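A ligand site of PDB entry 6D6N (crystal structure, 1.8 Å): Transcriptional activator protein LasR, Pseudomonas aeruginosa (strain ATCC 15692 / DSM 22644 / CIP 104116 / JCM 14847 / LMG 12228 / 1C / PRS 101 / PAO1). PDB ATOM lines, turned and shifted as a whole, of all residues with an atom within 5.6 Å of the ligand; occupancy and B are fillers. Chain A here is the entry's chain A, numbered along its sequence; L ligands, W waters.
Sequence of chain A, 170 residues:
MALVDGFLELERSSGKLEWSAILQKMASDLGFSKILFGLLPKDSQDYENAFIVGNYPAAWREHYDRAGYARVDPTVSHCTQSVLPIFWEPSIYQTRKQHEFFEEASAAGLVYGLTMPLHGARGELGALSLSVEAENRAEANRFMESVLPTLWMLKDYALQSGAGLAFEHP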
ATOM      1  N   LEU A  36     -13.242   8.116 -21.481  1.00  0.00           N
ATOM      2  CA  LEU A  36     -13.608   7.080 -22.429  1.00  0.00           C
ATOM      3  C   LEU A  36     -13.730   7.747 -23.811  1.00  0.00           C
ATOM      4  O   LEU A  36     -14.487   8.705 -23.972  1.00  0.00           O
ATOM      5  CB  LEU A  36     -14.911   6.452 -22.058  1.00  0.00           C
ATOM      6  CG  LEU A  36     -15.226   5.149 -22.719  1.00  0.00           C
ATOM      7  CD1 LEU A  36     -14.193   4.114 -22.220  1.00  0.00           C
ATOM      8  CD2 LEU A  36     -16.687   4.728 -22.512  1.00  0.00           C
ATOM      9  N   PHE A  37     -13.011   7.206 -24.796  1.00  0.00           N
ATOM     10  CA  PHE A  37     -13.096   7.647 -26.180  1.00  0.00           C
ATOM     11  C   PHE A  37     -13.790   6.543 -26.954  1.00  0.00           C
ATOM     12  O   PHE A  37     -13.316   5.386 -26.943  1.00  0.00           O
ATOM     13  CB  PHE A  37     -11.665   7.875 -26.729  1.00  0.00           C
ATOM     14  CG  PHE A  37     -11.602   8.262 -28.180  1.00  0.00           C
ATOM     15  CD1 PHE A  37     -11.582   7.249 -29.174  1.00  0.00           C
ATOM     16  CD2 PHE A  37     -11.507   9.586 -28.564  1.00  0.00           C
ATOM     17  CE1 PHE A  37     -11.452   7.651 -30.537  1.00  0.00           C
ATOM     18  CE2 PHE A  37     -11.378   9.976 -29.893  1.00  0.00           C
ATOM     19  CZ  PHE A  37     -11.366   8.990 -30.884  1.00  0.00           C
ATOM     20  N   GLY A  38     -14.943   6.862 -27.596  1.00  0.00           N
ATOM     21  CA  GLY A  38     -15.622   5.886 -28.420  1.00  0.00           C
ATOM     22  C   GLY A  38     -15.972   6.475 -29.742  1.00  0.00           C
ATOM     23  O   GLY A  38     -16.407   7.637 -29.820  1.00  0.00           O
ATOM     24  N   LEU A  39     -15.821   5.668 -30.793  1.00  0.00           N
ATOM     25  CA  LEU A  39     -15.961   6.142 -32.142  1.00  0.00           C
ATOM     26  C   LEU A  39     -16.540   4.999 -33.004  1.00  0.00           C
ATOM     27  O   LEU A  39     -16.101   3.857 -32.836  1.00  0.00           O
ATOM     28  CB  LEU A  39     -14.591   6.574 -32.629  1.00  0.00           C
ATOM     29  CG  LEU A  39     -14.628   7.437 -33.858  1.00  0.00           C
ATOM     30  CD1 LEU A  39     -15.334   8.788 -33.523  1.00  0.00           C
ATOM     31  CD2 LEU A  39     -13.262   7.696 -34.451  1.00  0.00           C
ATOM     32  N   LEU A  40     -17.595   5.302 -33.718  1.00  0.00           N
ATOM     33  CA  LEU A  40     -18.284   4.374 -34.643  1.00  0.00           C
ATOM     34  C   LEU A  40     -18.034   4.804 -36.091  1.00  0.00           C
ATOM     35  O   LEU A  40     -18.008   5.988 -36.396  1.00  0.00           O
ATOM     36  CB  LEU A  40     -19.787   4.443 -34.437  1.00  0.00           C
ATOM     37  CG  LEU A  40     -20.373   4.026 -33.068  1.00  0.00           C
ATOM     38  CD1 LEU A  40     -21.678   4.766 -32.762  1.00  0.00           C
ATOM     39  CD2 LEU A  40     -20.685   2.574 -33.069  1.00  0.00           C
ATOM     40  N   TYR A  47     -23.220  -1.252 -32.121  1.00  0.00           N
ATOM     41  CA  TYR A  47     -21.899  -0.976 -31.551  1.00  0.00           C
ATOM     42  C   TYR A  47     -20.908  -2.049 -31.831  1.00  0.00           C
ATOM     43  O   TYR A  47     -19.800  -2.030 -31.271  1.00  0.00           O
ATOM     44  CB  TYR A  47     -21.998  -0.741 -30.016  1.00  0.00           C
ATOM     45  CG  TYR A  47     -22.731   0.515 -29.684  1.00  0.00           C
ATOM     46  CD1 TYR A  47     -24.127   0.571 -29.713  1.00  0.00           C
ATOM     47  CD2 TYR A  47     -22.024   1.670 -29.339  1.00  0.00           C
ATOM     48  CE1 TYR A  47     -24.794   1.764 -29.442  1.00  0.00           C
ATOM     49  CE2 TYR A  47     -22.688   2.858 -29.076  1.00  0.00           C
ATOM     50  CZ  TYR A  47     -24.056   2.884 -29.100  1.00  0.00           C
ATOM     51  OH  TYR A  47     -24.669   4.070 -28.832  1.00  0.00           O
ATOM     52  N   ILE A  52     -13.505   1.659 -28.776  1.00  0.00           N
ATOM     53  CA  ILE A  52     -13.781   2.241 -27.448  1.00  0.00           C
ATOM     54  C   ILE A  52     -12.588   1.990 -26.613  1.00  0.00           C
ATOM     55  O   ILE A  52     -12.233   0.800 -26.424  1.00  0.00           O
ATOM     56  CB  ILE A  52     -15.019   1.637 -26.831  1.00  0.00           C
ATOM     57  CG1 ILE A  52     -16.209   1.868 -27.727  1.00  0.00           C
ATOM     58  CG2 ILE A  52     -15.258   2.280 -25.433  1.00  0.00           C
ATOM     59  CD1 ILE A  52     -17.470   1.103 -27.410  1.00  0.00           C
ATOM     60  N   TYR A  56     -12.082   4.035 -17.917  1.00  0.00           N
ATOM     61  CA  TYR A  56     -13.260   3.741 -17.110  1.00  0.00           C
ATOM     62  C   TYR A  56     -13.128   2.327 -16.460  1.00  0.00           C
ATOM     63  O   TYR A  56     -12.648   1.376 -17.121  1.00  0.00           O
ATOM     64  CB  TYR A  56     -14.554   3.759 -17.897  1.00  0.00           C
ATOM     65  CG  TYR A  56     -15.183   5.139 -18.197  1.00  0.00           C
ATOM     66  CD1 TYR A  56     -14.474   6.359 -18.066  1.00  0.00           C
ATOM     67  CD2 TYR A  56     -16.482   5.216 -18.595  1.00  0.00           C
ATOM     68  CE1 TYR A  56     -15.075   7.596 -18.292  1.00  0.00           C
ATOM     69  CE2 TYR A  56     -17.068   6.457 -18.870  1.00  0.00           C
ATOM     70  CZ  TYR A  56     -16.370   7.617 -18.698  1.00  0.00           C
ATOM     71  OH  TYR A  56     -17.009   8.847 -18.943  1.00  0.00           O
ATOM     72  N   TRP A  60     -18.029  -1.046 -14.493  1.00  0.00           N
ATOM     73  CA  TRP A  60     -18.950  -0.017 -15.040  1.00  0.00           C
ATOM     74  C   TRP A  60     -19.189  -0.245 -16.549  1.00  0.00           C
ATOM     75  O   TRP A  60     -20.353  -0.144 -17.074  1.00  0.00           O
ATOM     76  CB  TRP A  60     -18.419   1.388 -14.717  1.00  0.00           C
ATOM     77  CG  TRP A  60     -19.276   2.530 -15.262  1.00  0.00           C
ATOM     78  CD1 TRP A  60     -18.863   3.495 -16.088  1.00  0.00           C
ATOM     79  CD2 TRP A  60     -20.696   2.702 -15.103  1.00  0.00           C
ATOM     80  NE1 TRP A  60     -19.921   4.367 -16.398  1.00  0.00           N
ATOM     81  CE2 TRP A  60     -21.058   3.878 -15.833  1.00  0.00           C
ATOM     82  CE3 TRP A  60     -21.676   2.017 -14.395  1.00  0.00           C
ATOM     83  CZ2 TRP A  60     -22.355   4.395 -15.847  1.00  0.00           C
ATOM     84  CZ3 TRP A  60     -22.993   2.451 -14.496  1.00  0.00           C
ATOM     85  CH2 TRP A  60     -23.322   3.656 -15.211  1.00  0.00           C
ATOM     86  N   ARG A  61     -18.102  -0.442 -17.296  1.00  0.00           N
ATOM     87  CA  ARG A  61     -18.252  -0.764 -18.746  1.00  0.00           C
ATOM     88  C   ARG A  61     -19.155  -1.953 -18.963  1.00  0.00           C
ATOM     89  O   ARG A  61     -20.056  -1.954 -19.853  1.00  0.00           O
ATOM     90  CB  ARG A  61     -16.898  -1.053 -19.352  1.00  0.00           C
ATOM     91  CG  ARG A  61     -15.924   0.127 -19.489  1.00  0.00           C
ATOM     92  CD  ARG A  61     -16.242   1.117 -20.581  1.00  0.00           C
ATOM     93  NE  ARG A  61     -16.369   0.408 -21.845  1.00  0.00           N
ATOM     94  CZ  ARG A  61     -15.361  -0.048 -22.581  1.00  0.00           C
ATOM     95  NH1 ARG A  61     -15.629  -0.707 -23.670  1.00  0.00           N
ATOM     96  NH2 ARG A  61     -14.114   0.139 -22.227  1.00  0.00           N
ATOM     97  N   TYR A  64     -22.861  -1.075 -18.021  1.00  0.00           N
ATOM     98  CA  TYR A  64     -23.477  -0.144 -18.949  1.00  0.00           C
ATOM     99  C   TYR A  64     -23.969  -0.869 -20.177  1.00  0.00           C
ATOM    100  O   TYR A  64     -25.025  -0.583 -20.699  1.00  0.00           O
ATOM    101  CB  TYR A  64     -22.485   0.993 -19.291  1.00  0.00           C
ATOM    102  CG  TYR A  64     -22.922   2.113 -20.210  1.00  0.00           C
ATOM    103  CD1 TYR A  64     -23.019   1.916 -21.593  1.00  0.00           C
ATOM    104  CD2 TYR A  64     -23.177   3.378 -19.731  1.00  0.00           C
ATOM    105  CE1 TYR A  64     -23.359   2.942 -22.437  1.00  0.00           C
ATOM    106  CE2 TYR A  64     -23.513   4.437 -20.584  1.00  0.00           C
ATOM    107  CZ  TYR A  64     -23.595   4.202 -21.935  1.00  0.00           C
ATOM    108  OH  TYR A  64     -23.941   5.176 -22.781  1.00  0.00           O
ATOM    109  N   ASP A  65     -23.126  -1.758 -20.715  1.00  0.00           N
ATOM    110  CA  ASP A  65     -23.511  -2.564 -21.888  1.00  0.00           C
ATOM    111  C   ASP A  65     -24.684  -3.512 -21.562  1.00  0.00           C
ATOM    112  O   ASP A  65     -25.706  -3.549 -22.261  1.00  0.00           O
ATOM    113  CB  ASP A  65     -22.299  -3.382 -22.360  1.00  0.00           C
ATOM    114  CG  ASP A  65     -21.207  -2.518 -23.008  1.00  0.00           C
ATOM    115  OD1 ASP A  65     -21.398  -1.299 -23.306  1.00  0.00           O
ATOM    116  OD2 ASP A  65     -20.137  -3.091 -23.282  1.00  0.00           O
ATOM    117  N   ASP A  73     -28.734   6.826 -21.435  1.00  0.00           N
ATOM    118  CA  ASP A  73     -27.768   7.910 -21.249  1.00  0.00           C
ATOM    119  C   ASP A  73     -28.049   9.135 -22.130  1.00  0.00           C
ATOM    120  O   ASP A  73     -28.036   9.074 -23.359  1.00  0.00           O
ATOM    121  CB  ASP A  73     -26.382   7.294 -21.544  1.00  0.00           C
ATOM    122  CG  ASP A  73     -25.212   8.269 -21.507  1.00  0.00           C
ATOM    123  OD1 ASP A  73     -25.341   9.491 -21.339  1.00  0.00           O
ATOM    124  OD2 ASP A  73     -24.100   7.706 -21.646  1.00  0.00           O
ATOM    125  N   THR A  75     -26.415  11.767 -22.843  1.00  0.00           N
ATOM    126  CA  THR A  75     -25.307  12.300 -23.591  1.00  0.00           C
ATOM    127  C   THR A  75     -25.242  11.683 -24.987  1.00  0.00           C
ATOM    128  O   THR A  75     -24.707  12.337 -25.893  1.00  0.00           O
ATOM    129  CB  THR A  75     -23.961  12.130 -22.894  1.00  0.00           C
ATOM    130  OG1 THR A  75     -23.542  10.745 -22.888  1.00  0.00           O
ATOM    131  CG2 THR A  75     -23.963  12.660 -21.491  1.00  0.00           C
ATOM    132  N   VAL A  76     -25.684  10.422 -25.093  1.00  0.00           N
ATOM    133  CA  VAL A  76     -25.641   9.701 -26.357  1.00  0.00           C
ATOM    134  C   VAL A  76     -26.583  10.370 -27.377  1.00  0.00           C
ATOM    135  O   VAL A  76     -26.176  10.662 -28.494  1.00  0.00           O
ATOM    136  CB  VAL A  76     -25.963   8.213 -26.220  1.00  0.00           C
ATOM    137  CG1 VAL A  76     -26.031   7.554 -27.628  1.00  0.00           C
ATOM    138  CG2 VAL A  76     -24.928   7.517 -25.367  1.00  0.00           C
ATOM    139  N   CYS A  79     -25.182  13.723 -28.513  1.00  0.00           N
ATOM    140  CA  CYS A  79     -24.081  13.608 -29.519  1.00  0.00           C
ATOM    141  C   CYS A  79     -24.605  13.440 -30.959  1.00  0.00           C
ATOM    142  O   CYS A  79     -23.982  13.903 -31.914  1.00  0.00           O
ATOM    143  CB  CYS A  79     -23.139  12.461 -29.211  1.00  0.00           C
ATOM    144  SG  CYS A  79     -22.101  12.695 -27.769  1.00  0.00           S
ATOM    145  N   THR A  80     -25.744  12.770 -31.119  1.00  0.00           N
ATOM    146  CA  THR A  80     -26.325  12.576 -32.468  1.00  0.00           C
ATOM    147  C   THR A  80     -26.903  13.839 -33.076  1.00  0.00           C
ATOM    148  O   THR A  80     -27.160  13.895 -34.298  1.00  0.00           O
ATOM    149  CB  THR A  80     -27.452  11.509 -32.500  1.00  0.00           C
ATOM    150  OG1 THR A  80     -28.620  12.018 -31.828  1.00  0.00           O
ATOM    151  CG2 THR A  80     -26.984  10.204 -31.924  1.00  0.00           C
ATOM    152  N   TRP A  88     -22.389  16.720 -17.422  1.00  0.00           N
ATOM    153  CA  TRP A  88     -23.134  15.626 -16.827  1.00  0.00           C
ATOM    154  C   TRP A  88     -23.972  16.179 -15.671  1.00  0.00           C
ATOM    155  O   TRP A  88     -23.415  16.557 -14.655  1.00  0.00           O
ATOM    156  CB  TRP A  88     -22.205  14.606 -16.271  1.00  0.00           C
ATOM    157  CG  TRP A  88     -21.342  13.904 -17.245  1.00  0.00           C
ATOM    158  CD1 TRP A  88     -21.378  14.014 -18.590  1.00  0.00           C
ATOM    159  CD2 TRP A  88     -20.342  12.970 -16.921  1.00  0.00           C
ATOM    160  NE1 TRP A  88     -20.393  13.233 -19.149  1.00  0.00           N
ATOM    161  CE2 TRP A  88     -19.757  12.549 -18.152  1.00  0.00           C
ATOM    162  CE3 TRP A  88     -19.864  12.431 -15.723  1.00  0.00           C
ATOM    163  CZ2 TRP A  88     -18.747  11.607 -18.201  1.00  0.00           C
ATOM    164  CZ3 TRP A  88     -18.858  11.538 -15.758  1.00  0.00           C
ATOM    165  CH2 TRP A  88     -18.315  11.093 -17.011  1.00  0.00           C
ATOM    166  N   PHE A 101     -29.629   5.285 -14.183  1.00  0.00           N
ATOM    167  CA  PHE A 101     -28.325   5.545 -14.861  1.00  0.00           C
ATOM    168  C   PHE A 101     -27.477   6.489 -14.061  1.00  0.00           C
ATOM    169  O   PHE A 101     -26.364   6.153 -13.713  1.00  0.00           O
ATOM    170  CB  PHE A 101     -28.512   6.082 -16.283  1.00  0.00           C
ATOM    171  CG  PHE A 101     -27.236   6.613 -16.886  1.00  0.00           C
ATOM    172  CD1 PHE A 101     -26.246   5.759 -17.262  1.00  0.00           C
ATOM    173  CD2 PHE A 101     -27.031   7.971 -17.068  1.00  0.00           C
ATOM    174  CE1 PHE A 101     -25.030   6.231 -17.765  1.00  0.00           C
ATOM    175  CE2 PHE A 101     -25.833   8.451 -17.607  1.00  0.00           C
ATOM    176  CZ  PHE A 101     -24.830   7.575 -17.963  1.00  0.00           C
ATOM    177  N   PHE A 102     -28.027   7.647 -13.662  1.00  0.00           N
ATOM    178  CA  PHE A 102     -27.179   8.593 -12.877  1.00  0.00           C
ATOM    179  C   PHE A 102     -26.771   8.008 -11.527  1.00  0.00           C
ATOM    180  O   PHE A 102     -25.660   8.199 -11.091  1.00  0.00           O
ATOM    181  CB  PHE A 102     -27.771   9.982 -12.763  1.00  0.00           C
ATOM    182  CG  PHE A 102     -27.584  10.790 -14.007  1.00  0.00           C
ATOM    183  CD1 PHE A 102     -26.341  11.379 -14.317  1.00  0.00           C
ATOM    184  CD2 PHE A 102     -28.648  10.947 -14.924  1.00  0.00           C
ATOM    185  CE1 PHE A 102     -26.187  12.119 -15.497  1.00  0.00           C
ATOM    186  CE2 PHE A 102     -28.517  11.676 -16.065  1.00  0.00           C
ATOM    187  CZ  PHE A 102     -27.260  12.243 -16.355  1.00  0.00           C
ATOM    188  N   ALA A 105     -23.952   5.356 -12.229  1.00  0.00           N
ATOM    189  CA  ALA A 105     -22.705   6.084 -12.524  1.00  0.00           C
ATOM    190  C   ALA A 105     -22.022   6.658 -11.265  1.00  0.00           C
ATOM    191  O   ALA A 105     -20.794   6.547 -11.045  1.00  0.00           O
ATOM    192  CB  ALA A 105     -22.919   7.180 -13.583  1.00  0.00           C
ATOM    193  N   LEU A 110     -18.272   7.994 -11.045  1.00  0.00           N
ATOM    194  CA  LEU A 110     -18.371   8.904 -12.136  1.00  0.00           C
ATOM    195  C   LEU A 110     -19.561   9.824 -11.949  1.00  0.00           C
ATOM    196  O   LEU A 110     -20.672   9.551 -12.376  1.00  0.00           O
ATOM    197  CB  LEU A 110     -18.496   8.092 -13.451  1.00  0.00           C
ATOM    198  CG  LEU A 110     -17.144   7.425 -13.706  1.00  0.00           C
ATOM    199  CD1 LEU A 110     -17.237   5.978 -13.333  1.00  0.00           C
ATOM    200  CD2 LEU A 110     -16.742   7.516 -15.177  1.00  0.00           C
ATOM    201  N   THR A 115     -19.315  15.288 -21.756  1.00  0.00           N
ATOM    202  CA  THR A 115     -19.165  14.451 -22.977  1.00  0.00           C
ATOM    203  C   THR A 115     -19.000  15.439 -24.168  1.00  0.00           C
ATOM    204  O   THR A 115     -19.826  16.359 -24.363  1.00  0.00           O
ATOM    205  CB  THR A 115     -20.332  13.490 -23.062  1.00  0.00           C
ATOM    206  OG1 THR A 115     -20.318  12.550 -21.977  1.00  0.00           O
ATOM    207  CG2 THR A 115     -20.262  12.752 -24.419  1.00  0.00           C
ATOM    208  N   LEU A 125     -18.818   8.840 -35.998  1.00  0.00           N
ATOM    209  CA  LEU A 125     -19.651   9.377 -34.931  1.00  0.00           C
ATOM    210  C   LEU A 125     -19.145   8.891 -33.571  1.00  0.00           C
ATOM    211  O   LEU A 125     -18.987   7.681 -33.354  1.00  0.00           O
ATOM    212  CB  LEU A 125     -21.092   8.997 -35.182  1.00  0.00           C
ATOM    213  CG  LEU A 125     -22.109   9.201 -34.047  1.00  0.00           C
ATOM    214  CD1 LEU A 125     -22.228  10.653 -33.699  1.00  0.00           C
ATOM    215  CD2 LEU A 125     -23.497   8.542 -34.308  1.00  0.00           C
ATOM    216  N   GLY A 126     -18.981   9.765 -32.595  1.00  0.00           N
ATOM    217  CA  GLY A 126     -18.583   9.243 -31.294  1.00  0.00           C
ATOM    218  C   GLY A 126     -18.578  10.283 -30.222  1.00  0.00           C
ATOM    219  O   GLY A 126     -19.303  11.240 -30.309  1.00  0.00           O
ATOM    220  N   ALA A 127     -17.802  10.009 -29.185  1.00  0.00           N
ATOM    221  CA  ALA A 127     -17.744  10.864 -27.999  1.00  0.00           C
ATOM    222  C   ALA A 127     -16.456  10.713 -27.219  1.00  0.00           C
ATOM    223  O   ALA A 127     -15.944   9.597 -27.098  1.00  0.00           O
ATOM    224  CB  ALA A 127     -18.948  10.517 -27.124  1.00  0.00           C
ATOM    225  N   SER A 129     -15.675  11.276 -23.402  1.00  0.00           N
ATOM    226  CA  SER A 129     -16.334  11.505 -22.107  1.00  0.00           C
ATOM    227  C   SER A 129     -15.254  11.580 -21.059  1.00  0.00           C
ATOM    228  O   SER A 129     -14.353  10.805 -21.086  1.00  0.00           O
ATOM    229  CB  SER A 129     -17.265  10.382 -21.857  1.00  0.00           C
ATOM    230  OG  SER A 129     -18.351  10.528 -22.734  1.00  0.00           O
HETATM  231  C1  LIG L   1     -20.129   3.719 -23.242  1.00  0.00           C
HETATM  232  C2  LIG L   1     -20.265   6.350 -26.839  1.00  0.00           C
HETATM  233  C3  LIG L   1     -19.894   6.649 -29.251  1.00  0.00           C
HETATM  234  C4  LIG L   1     -22.644   8.270 -30.741  1.00  0.00           C
HETATM  235  C5  LIG L   1     -22.148   6.683 -28.352  1.00  0.00           C
HETATM  236  C6  LIG L   1     -21.626   6.464 -27.079  1.00  0.00           C
HETATM  237  C7  LIG L   1     -21.378   9.093 -19.058  1.00  0.00           C
HETATM  238  O1  LIG L   1     -19.373   8.460 -20.137  1.00  0.00           O
HETATM  239  C8  LIG L   1     -20.666   8.441 -20.168  1.00  0.00           C
HETATM  240  N1  LIG L   1     -21.377   7.957 -21.157  1.00  0.00           N
HETATM  241  C9  LIG L   1     -20.792   7.346 -22.403  1.00  0.00           C
HETATM  242  C10 LIG L   1     -20.432   5.856 -22.224  1.00  0.00           C
HETATM  243  C11 LIG L   1     -20.113   5.252 -21.030  1.00  0.00           C
HETATM  244  C12 LIG L   1     -19.840   3.812 -20.916  1.00  0.00           C
HETATM  245 BR1  LIG L   1     -19.528   3.053 -19.444  1.00  0.00          BR
HETATM  246  C13 LIG L   1     -19.813   3.033 -22.104  1.00  0.00           C
HETATM  247 BR2  LIG L   1     -20.197   2.775 -24.967  1.00  0.00          BR
HETATM  248  C14 LIG L   1     -20.388   5.067 -23.362  1.00  0.00           C
HETATM  249  O2  LIG L   1     -20.730   5.687 -24.498  1.00  0.00           O
HETATM  250  C15 LIG L   1     -19.838   6.087 -25.474  1.00  0.00           C
HETATM  251  C16 LIG L   1     -19.423   6.506 -27.986  1.00  0.00           C
HETATM  252  C17 LIG L   1     -21.248   6.809 -29.483  1.00  0.00           C
HETATM  253  O3  LIG L   1     -21.731   7.052 -30.699  1.00  0.00           O
HETATM  254  O4  LIG L   1     -18.686   6.096 -25.149  1.00  0.00           O
HETATM  255  C18 LIG L   1     -21.247   8.827 -17.735  1.00  0.00           C
HETATM  256  N2  LIG L   1     -20.448   7.628 -17.269  1.00  0.00           N
HETATM  257  O5  LIG L   1     -20.428   6.671 -18.061  1.00  0.00           O
HETATM  258  O6  LIG L   1     -19.964   7.545 -16.209  1.00  0.00           O
HETATM  259  C19 LIG L   1     -21.891   9.529 -16.690  1.00  0.00           C
HETATM  260  C20 LIG L   1     -22.713  10.587 -17.022  1.00  0.00           C
HETATM  261  C21 LIG L   1     -22.880  10.909 -18.346  1.00  0.00           C
HETATM  262  C22 LIG L   1     -22.197  10.217 -19.386  1.00  0.00           C
HETATM  263  O   HOH W   1     -19.335  -0.235 -22.100  1.00  0.00           O
HETATM  264  O   HOH W   2     -17.520   8.523 -24.458  1.00  0.00           O
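Water W1 lies within hydrogen-bond range of OD1 of Asp 65 (2.6 Å) and O of Arg 61 (2.9 Å).
The side-chain carboxylate (OD2) of Asp 73 sits at hydrogen-bond distance from the side-chain hydroxyl (OH) of Tyr 64 (2.8 Å).
The side-chain carboxylate (OD1) of Asp 73 lies within hydrogen-bond range of the side-chain hydroxyl (OG1) of Thr 75, at 2.7 Å.
The backbone carbonyl oxygen (O) of Leu 125 is in hydrogen-bond range of the backbone NH (N) of Leu 40, at 2.8 Å.
O of Leu 36 sits at hydrogen-bond distance from N of Ser 129, at 2.9 Å.
The side-chain hydroxyl (OG1) of Thr 115 is in hydrogen-bond range of the side-chain hydroxyl (OG) of Ser 129 (2.9 Å).
The side-chain hydroxyl (OG1) of Thr 115 sits at hydrogen-bond distance from the indole nitrogen (NE1) of Trp 88 (2.9 Å).
The backbone NH (N) of Ala 127 is in hydrogen-bond range of the backbone carbonyl oxygen (O) of Gly 38 (2.8 Å).
The side-chain sulfur (SG) of Cys 79 is in hydrogen-bond range of the backbone carbonyl oxygen (O) of Thr 75 (3.2 Å).
OH of Tyr 56 is in hydrogen-bond range of O1 of the ligand, 2.7 Å away.
A nitrogen (N1) of the ligand sits at hydrogen-bond distance from the side-chain carboxylate of Asp 73 (2.8 Å).
O5 of the ligand is in hydrogen-bond range of NE1 of Trp 60, 2.9 Å away.
The side-chain hydroxyl of Ser 129 sits close to an oxygen (O1) of the ligand.
Merely in contact with the ligand: Leu 36 (3.6 Å), Gly 38 (3.7 Å), Leu 40 (3.1 Å), Tyr 47 (3.7 Å), Arg 61 (3.98 Å), Tyr 64 (3.4 Å), Thr 75 (3.7 Å), Val 76 (3.9 Å), Trp 88 (3.4 Å), Phe 101 (3.8 Å), Ala 105 (3.97 Å), Leu 110 (3.2 Å), Thr 115 (3.96 Å), Leu 125 (3.5 Å), Gly 126 (3.6 Å) and Ala 127 (3.96 Å).
Hydrophobic or aromatic side chains that line the ligand: Leu 36, Leu 40, Tyr 47, Tyr 56, Trp 60, Tyr 64, Val 76, Trp 88, Phe 101, Ala 105, Leu 110 and Leu 125.
Within 4 Å of the ligand: Leu 36, Gly 38, Leu 40, Tyr 47, Tyr 56, Trp 60, Arg 61, Tyr 64, Asp 73, Thr 75, Val 76, Trp 88, Phe 101, Ala 105, Leu 110, Thr 115, Leu 125, Gly 126, Ala 127 and Ser 129.
The nearest printed residue that does not touch the ligand is Ile 52 (4.02 Å).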
